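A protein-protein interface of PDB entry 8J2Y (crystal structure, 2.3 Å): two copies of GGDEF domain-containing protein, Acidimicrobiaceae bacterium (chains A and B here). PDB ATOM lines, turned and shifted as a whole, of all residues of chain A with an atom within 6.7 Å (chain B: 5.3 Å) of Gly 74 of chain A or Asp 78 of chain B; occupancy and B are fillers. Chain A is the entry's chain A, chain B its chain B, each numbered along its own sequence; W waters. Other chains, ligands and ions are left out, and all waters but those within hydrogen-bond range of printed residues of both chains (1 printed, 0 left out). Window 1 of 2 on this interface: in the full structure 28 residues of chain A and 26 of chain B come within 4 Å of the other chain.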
ATOM      1  N   TYR A  11       7.441 -38.689 -15.470  1.00  0.00           N
ATOM      2  CA  TYR A  11       7.346 -37.531 -14.597  1.00  0.00           C
ATOM      3  C   TYR A  11       6.407 -36.486 -15.202  1.00  0.00           C
ATOM      4  O   TYR A  11       5.487 -36.046 -14.518  1.00  0.00           O
ATOM      5  CB  TYR A  11       8.730 -36.893 -14.280  1.00  0.00           C
ATOM      6  CG  TYR A  11       8.632 -35.541 -13.593  1.00  0.00           C
ATOM      7  CD1 TYR A  11       8.491 -34.372 -14.331  1.00  0.00           C
ATOM      8  CD2 TYR A  11       8.665 -35.434 -12.200  1.00  0.00           C
ATOM      9  CE1 TYR A  11       8.388 -33.126 -13.709  1.00  0.00           C
ATOM     10  CE2 TYR A  11       8.566 -34.191 -11.564  1.00  0.00           C
ATOM     11  CZ  TYR A  11       8.425 -33.034 -12.320  1.00  0.00           C
ATOM     12  OH  TYR A  11       8.313 -31.794 -11.696  1.00  0.00           O
ATOM     13  N   ARG A  20       0.599 -34.248  -8.633  1.00  0.00           N
ATOM     14  CA  ARG A  20       1.800 -34.045  -7.847  1.00  0.00           C
ATOM     15  C   ARG A  20       2.408 -35.300  -7.227  1.00  0.00           C
ATOM     16  O   ARG A  20       3.615 -35.495  -7.270  1.00  0.00           O
ATOM     17  CB  ARG A  20       1.389 -33.058  -6.759  1.00  0.00           C
ATOM     18  CG  ARG A  20       2.396 -32.732  -5.729  1.00  0.00           C
ATOM     19  CD  ARG A  20       1.752 -31.884  -4.699  1.00  0.00           C
ATOM     20  NE  ARG A  20       1.327 -30.603  -5.230  1.00  0.00           N
ATOM     21  CZ  ARG A  20       1.612 -29.461  -4.634  1.00  0.00           C
ATOM     22  NH1 ARG A  20       2.106 -29.431  -3.408  1.00  0.00           N
ATOM     23  NH2 ARG A  20       1.420 -28.321  -5.285  1.00  0.00           N
ATOM     24  N   VAL A  24       6.342 -36.462  -7.400  1.00  0.00           N
ATOM     25  CA  VAL A  24       7.229 -36.199  -6.271  1.00  0.00           C
ATOM     26  C   VAL A  24       7.793 -37.521  -5.739  1.00  0.00           C
ATOM     27  O   VAL A  24       8.923 -37.593  -5.244  1.00  0.00           O
ATOM     28  CB  VAL A  24       6.488 -35.384  -5.135  1.00  0.00           C
ATOM     29  CG1 VAL A  24       7.255 -35.397  -3.825  1.00  0.00           C
ATOM     30  CG2 VAL A  24       6.193 -33.948  -5.558  1.00  0.00           C
ATOM     31  N   ALA A  69       2.674 -28.062 -14.118  1.00  0.00           N
ATOM     32  CA  ALA A  69       3.993 -28.677 -14.102  1.00  0.00           C
ATOM     33  C   ALA A  69       4.944 -27.935 -13.158  1.00  0.00           C
ATOM     34  O   ALA A  69       5.677 -28.552 -12.383  1.00  0.00           O
ATOM     35  CB  ALA A  69       4.529 -28.753 -15.509  1.00  0.00           C
ATOM     36  N   SER A  70       4.884 -26.601 -13.151  1.00  0.00           N
ATOM     37  CA  SER A  70       5.810 -25.832 -12.342  1.00  0.00           C
ATOM     38  C   SER A  70       5.508 -25.971 -10.852  1.00  0.00           C
ATOM     39  O   SER A  70       6.420 -25.959 -10.014  1.00  0.00           O
ATOM     40  CB  SER A  70       5.841 -24.361 -12.765  1.00  0.00           C
ATOM     41  OG  SER A  70       6.407 -24.179 -14.070  1.00  0.00           O
ATOM     42  N   GLY A  71       4.223 -26.130 -10.505  1.00  0.00           N
ATOM     43  CA  GLY A  71       3.874 -26.365  -9.114  1.00  0.00           C
ATOM     44  C   GLY A  71       4.434 -27.709  -8.642  1.00  0.00           C
ATOM     45  O   GLY A  71       4.935 -27.826  -7.511  1.00  0.00           O
ATOM     46  N   VAL A  72       4.349 -28.728  -9.515  1.00  0.00           N
ATOM     47  CA  VAL A  72       4.801 -30.067  -9.165  1.00  0.00           C
ATOM     48  C   VAL A  72       6.309 -30.053  -8.913  1.00  0.00           C
ATOM     49  O   VAL A  72       6.782 -30.693  -7.966  1.00  0.00           O
ATOM     50  CB  VAL A  72       4.389 -31.090 -10.268  1.00  0.00           C
ATOM     51  CG1 VAL A  72       4.939 -32.497  -9.992  1.00  0.00           C
ATOM     52  CG2 VAL A  72       2.879 -31.118 -10.456  1.00  0.00           C
ATOM     53  N   ALA A  73       7.033 -29.281  -9.739  1.00  0.00           N
ATOM     54  CA  ALA A  73       8.477 -29.174  -9.625  1.00  0.00           C
ATOM     55  C   ALA A  73       8.857 -28.511  -8.304  1.00  0.00           C
ATOM     56  O   ALA A  73       9.759 -28.974  -7.591  1.00  0.00           O
ATOM     57  CB  ALA A  73       9.046 -28.377 -10.823  1.00  0.00           C
ATOM     58  N   GLY A  74       8.146 -27.425  -7.968  1.00  0.00           N
ATOM     59  CA  GLY A  74       8.344 -26.785  -6.678  1.00  0.00           C
ATOM     60  C   GLY A  74       8.088 -27.752  -5.522  1.00  0.00           C
ATOM     61  O   GLY A  74       8.781 -27.717  -4.506  1.00  0.00           O
ATOM     62  N   ALA A  75       7.076 -28.617  -5.669  1.00  0.00           N
ATOM     63  CA  ALA A  75       6.740 -29.550  -4.597  1.00  0.00           C
ATOM     64  C   ALA A  75       7.774 -30.668  -4.467  1.00  0.00           C
ATOM     65  O   ALA A  75       8.043 -31.143  -3.361  1.00  0.00           O
ATOM     66  CB  ALA A  75       5.375 -30.141  -4.835  1.00  0.00           C
ATOM     67  N   ALA A  76       8.337 -31.084  -5.616  1.00  0.00           N
ATOM     68  CA  ALA A  76       9.464 -32.011  -5.658  1.00  0.00           C
ATOM     69  C   ALA A  76      10.701 -31.481  -4.926  1.00  0.00           C
ATOM     70  O   ALA A  76      11.282 -32.178  -4.094  1.00  0.00           O
ATOM     71  CB  ALA A  76       9.826 -32.353  -7.113  1.00  0.00           C
ATOM     72  N   LEU A  77      11.084 -30.241  -5.231  1.00  0.00           N
ATOM     73  CA  LEU A  77      12.177 -29.589  -4.522  1.00  0.00           C
ATOM     74  C   LEU A  77      11.936 -29.491  -3.021  1.00  0.00           C
ATOM     75  O   LEU A  77      12.834 -29.753  -2.233  1.00  0.00           O
ATOM     76  CB  LEU A  77      12.382 -28.182  -5.080  1.00  0.00           C
ATOM     77  CG  LEU A  77      12.974 -28.151  -6.465  1.00  0.00           C
ATOM     78  CD1 LEU A  77      12.998 -26.716  -6.993  1.00  0.00           C
ATOM     79  CD2 LEU A  77      14.377 -28.779  -6.476  1.00  0.00           C
ATOM     80  N   ASP A  78      10.711 -29.125  -2.639  1.00  0.00           N
ATOM     81  CA  ASP A  78      10.319 -29.107  -1.229  1.00  0.00           C
ATOM     82  C   ASP A  78      10.448 -30.467  -0.536  1.00  0.00           C
ATOM     83  O   ASP A  78      11.011 -30.543   0.548  1.00  0.00           O
ATOM     84  CB  ASP A  78       8.887 -28.511  -1.080  1.00  0.00           C
ATOM     85  CG  ASP A  78       8.859 -26.962  -1.193  1.00  0.00           C
ATOM     86  OD1 ASP A  78       9.939 -26.332  -1.071  1.00  0.00           O
ATOM     87  OD2 ASP A  78       7.759 -26.384  -1.444  1.00  0.00           O
ATOM     88  N   ALA A  79       9.954 -31.531  -1.180  1.00  0.00           N
ATOM     89  CA  ALA A  79      10.101 -32.883  -0.663  1.00  0.00           C
ATOM     90  C   ALA A  79      11.564 -33.275  -0.459  1.00  0.00           C
ATOM     91  O   ALA A  79      11.937 -33.802   0.594  1.00  0.00           O
ATOM     92  CB  ALA A  79       9.423 -33.870  -1.589  1.00  0.00           C
ATOM     93  N   LEU A 105      12.155 -20.954 -10.163  1.00  0.00           N
ATOM     94  CA  LEU A 105      12.678 -22.314 -10.215  1.00  0.00           C
ATOM     95  C   LEU A 105      14.135 -22.436 -10.680  1.00  0.00           C
ATOM     96  O   LEU A 105      14.811 -23.401 -10.337  1.00  0.00           O
ATOM     97  CB  LEU A 105      11.791 -23.165 -11.152  1.00  0.00           C
ATOM     98  CG  LEU A 105      10.399 -23.622 -10.516  1.00  0.00           C
ATOM     99  CD1 LEU A 105       9.445 -24.166 -11.563  1.00  0.00           C
ATOM    100  CD2 LEU A 105      10.605 -24.688  -9.403  1.00  0.00           C
ATOM    101  N   GLN A 108      15.910 -21.604  -7.478  1.00  0.00           N
ATOM    102  CA  GLN A 108      15.576 -22.633  -6.510  1.00  0.00           C
ATOM    103  C   GLN A 108      16.265 -23.953  -6.796  1.00  0.00           C
ATOM    104  O   GLN A 108      16.800 -24.572  -5.879  1.00  0.00           O
ATOM    105  CB  GLN A 108      14.052 -22.864  -6.461  1.00  0.00           C
ATOM    106  CG  GLN A 108      13.274 -21.744  -5.753  1.00  0.00           C
ATOM    107  CD  GLN A 108      11.767 -21.856  -5.941  1.00  0.00           C
ATOM    108  OE1 GLN A 108      11.280 -22.365  -6.928  1.00  0.00           O
ATOM    109  NE2 GLN A 108      10.981 -21.323  -5.007  1.00  0.00           N
ATOM    110  N   MET A 109      16.220 -24.381  -8.062  1.00  0.00           N
ATOM    111  CA  MET A 109      16.952 -25.567  -8.488  1.00  0.00           C
ATOM    112  C   MET A 109      18.451 -25.399  -8.227  1.00  0.00           C
ATOM    113  O   MET A 109      19.125 -26.302  -7.726  1.00  0.00           O
ATOM    114  CB  MET A 109      16.691 -25.848  -9.977  1.00  0.00           C
ATOM    115  CG  MET A 109      15.380 -26.582 -10.185  1.00  0.00           C
ATOM    116  SD  MET A 109      15.125 -27.143 -11.875  1.00  0.00           S
ATOM    117  CE  MET A 109      13.397 -27.399 -11.906  1.00  0.00           C
ATOM    118  N   ALA B  73       5.773 -20.746   3.525  1.00  0.00           N
ATOM    119  CA  ALA B  73       4.343 -20.945   3.415  1.00  0.00           C
ATOM    120  C   ALA B  73       4.025 -21.963   2.325  1.00  0.00           C
ATOM    121  O   ALA B  73       3.245 -22.900   2.531  1.00  0.00           O
ATOM    122  CB  ALA B  73       3.694 -19.616   3.131  1.00  0.00           C
ATOM    123  N   GLY B  74       4.669 -21.806   1.162  1.00  0.00           N
ATOM    124  CA  GLY B  74       4.485 -22.771   0.095  1.00  0.00           C
ATOM    125  C   GLY B  74       4.983 -24.150   0.510  1.00  0.00           C
ATOM    126  O   GLY B  74       4.424 -25.149   0.102  1.00  0.00           O
ATOM    127  N   ALA B  75       6.037 -24.221   1.323  1.00  0.00           N
ATOM    128  CA  ALA B  75       6.577 -25.504   1.746  1.00  0.00           C
ATOM    129  C   ALA B  75       5.664 -26.175   2.769  1.00  0.00           C
ATOM    130  O   ALA B  75       5.536 -27.403   2.781  1.00  0.00           O
ATOM    131  CB  ALA B  75       7.965 -25.322   2.319  1.00  0.00           C
ATOM    132  N   ALA B  76       5.024 -25.353   3.614  1.00  0.00           N
ATOM    133  CA  ALA B  76       4.003 -25.843   4.532  1.00  0.00           C
ATOM    134  C   ALA B  76       2.786 -26.428   3.813  1.00  0.00           C
ATOM    135  O   ALA B  76       2.333 -27.524   4.136  1.00  0.00           O
ATOM    136  CB  ALA B  76       3.592 -24.731   5.485  1.00  0.00           C
ATOM    137  N   LEU B  77       2.260 -25.705   2.819  1.00  0.00           N
ATOM    138  CA  LEU B  77       1.184 -26.222   1.983  1.00  0.00           C
ATOM    139  C   LEU B  77       1.557 -27.532   1.290  1.00  0.00           C
ATOM    140  O   LEU B  77       0.772 -28.472   1.241  1.00  0.00           O
ATOM    141  CB  LEU B  77       0.806 -25.172   0.961  1.00  0.00           C
ATOM    142  CG  LEU B  77       0.124 -23.973   1.522  1.00  0.00           C
ATOM    143  CD1 LEU B  77      -0.123 -22.939   0.473  1.00  0.00           C
ATOM    144  CD2 LEU B  77      -1.319 -24.411   2.240  1.00  0.00           C
ATOM    145  N   ASP B  78       2.781 -27.601   0.777  1.00  0.00           N
ATOM    146  CA  ASP B  78       3.285 -28.819   0.157  1.00  0.00           C
ATOM    147  C   ASP B  78       3.349 -30.004   1.119  1.00  0.00           C
ATOM    148  O   ASP B  78       2.942 -31.110   0.764  1.00  0.00           O
ATOM    149  CB  ASP B  78       4.682 -28.545  -0.517  1.00  0.00           C
ATOM    150  CG  ASP B  78       4.578 -27.811  -1.864  1.00  0.00           C
ATOM    151  OD1 ASP B  78       3.442 -27.695  -2.419  1.00  0.00           O
ATOM    152  OD2 ASP B  78       5.620 -27.367  -2.383  1.00  0.00           O
ATOM    153  N   ALA B  79       3.866 -29.761   2.331  1.00  0.00           N
ATOM    154  CA  ALA B  79       3.906 -30.771   3.377  1.00  0.00           C
ATOM    155  C   ALA B  79       2.510 -31.298   3.689  1.00  0.00           C
ATOM    156  O   ALA B  79       2.315 -32.512   3.743  1.00  0.00           O
ATOM    157  CB  ALA B  79       4.543 -30.207   4.625  1.00  0.00           C
ATOM    158  N   LEU B  80       1.570 -30.361   3.901  1.00  0.00           N
ATOM    159  CA  LEU B  80       0.176 -30.667   4.205  1.00  0.00           C
ATOM    160  C   LEU B  80      -0.449 -31.474   3.077  1.00  0.00           C
ATOM    161  O   LEU B  80      -1.126 -32.467   3.336  1.00  0.00           O
ATOM    162  CB  LEU B  80      -0.663 -29.399   4.373  1.00  0.00           C
ATOM    163  CG  LEU B  80      -0.333 -28.585   5.619  1.00  0.00           C
ATOM    164  CD1 LEU B  80      -1.029 -27.257   5.612  1.00  0.00           C
ATOM    165  CD2 LEU B  80      -0.717 -29.320   6.854  1.00  0.00           C
ATOM    166  N   ALA B  81      -0.182 -31.061   1.826  1.00  0.00           N
ATOM    167  CA  ALA B  81      -0.777 -31.764   0.702  1.00  0.00           C
ATOM    168  C   ALA B  81      -0.286 -33.213   0.622  1.00  0.00           C
ATOM    169  O   ALA B  81      -1.037 -34.114   0.231  1.00  0.00           O
ATOM    170  CB  ALA B  81      -0.557 -31.015  -0.579  1.00  0.00           C
ATOM    171  N   ALA B  82       0.951 -33.455   1.070  1.00  0.00           N
ATOM    172  CA  ALA B  82       1.509 -34.799   1.035  1.00  0.00           C
ATOM    173  C   ALA B  82       0.916 -35.702   2.118  1.00  0.00           C
ATOM    174  O   ALA B  82       1.111 -36.907   2.084  1.00  0.00           O
ATOM    175  CB  ALA B  82       3.028 -34.745   1.148  1.00  0.00           C
HETATM  176  O   HOH W   1       2.902 -31.533  -1.736  1.00  0.00           O
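The guanidinium group (NH1) of Arg 20 of chain A lies within salt-bridge range of the side-chain carboxylate (OD1) of Asp 78 of chain B.
The side-chain carboxylate (OD2) of Asp 78 of chain A lies close to the side-chain carboxylate (OD2) of Asp 78 of chain B (2.5 Å).
Among the printed residues, pairs that only touch across the chains: Ala 75 of chain A with Asp 78 of chain B (3.3 Å), Asp 78 of chain A with Ala 75 of chain B (3.5 Å), Gly 74 of chain A with Asp 78 of chain B (3.8 Å) and Asp 78 of chain A with Gly 74 of chain B (3.9 Å).
Printed residues of chain B within 4 Å of Arg 20 of chain A: Asp 78 (2.4 Å).
Printed residues of chain B within 4 Å of Ala 75 of chain A: Asp 78 (3.3 Å).
Leu 77 of chain A touches none of the printed residues of chain B.
Printed residues of chain B within 4 Å of Asp 78 of chain A: Gly 74 (3.9 Å), Ala 75 (3.5 Å) and Asp 78 (2.5 Å).
Printed residues of chain A within 4 Å of Gly 74 of chain B: Asp 78.
Printed residues of chain A within 4 Å of Ala 75 of chain B: Asp 78 (3.5 Å).
Printed residues of chain A within 4 Å of Asp 78 of chain B: Arg 20 (2.4 Å), Gly 74 (3.8 Å), Ala 75 (3.3 Å) and Asp 78 (2.5 Å).
Ala 81 of chain B touches none of the printed residues of chain A.
The nearest printed residue of chain A that does not touch Asp 78 of chain B is Gly 71 of chain A (5.2 Å).
Of the 10 printed residues of chain B, 3 touch a printed residue of chain A.
Of the 17 printed residues of chain A, 4 touch a printed residue of chain B.
Hydrophobic or aromatic side chains of chain A that line the printed part of chain B: Ala 75.
Along chain A the printed residues that touch a printed residue of chain B span positions 20 to 78.
Among the printed residues, 6 pairs touch across the chains.
Among the printed residues, Asp or Glu carboxylates within 4 Å of a Lys or Arg side-chain nitrogen of the other chain: Arg 20 of chain A with Asp 78 of chain B.
Gly 74 of chain A touches Asp 78 of chain B, and with the chains exchanged Asp 78 of chain A touches Gly 74 of chain B.
Ala 75 of chain A touches Asp 78 of chain B, and with the chains exchanged Asp 78 of chain A touches Ala 75 of chain B.
Asp 78 of chain A touches its own counterpart, Asp 78 of chain B.
Positions printed for both chains: 73, 74, 75, 76, 77, 78 and 79.
Of the 6 pairs that touch across the chains among the printed residues, 5 have their exchanged pair printed and touching as well.
Water W1 lies within hydrogen-bond range of the backbone carbonyl oxygen (O) of Asp 78 of chain B (2.5 Å) and the guanidinium group (NH1) of Arg 20 of chain A (2.8 Å).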
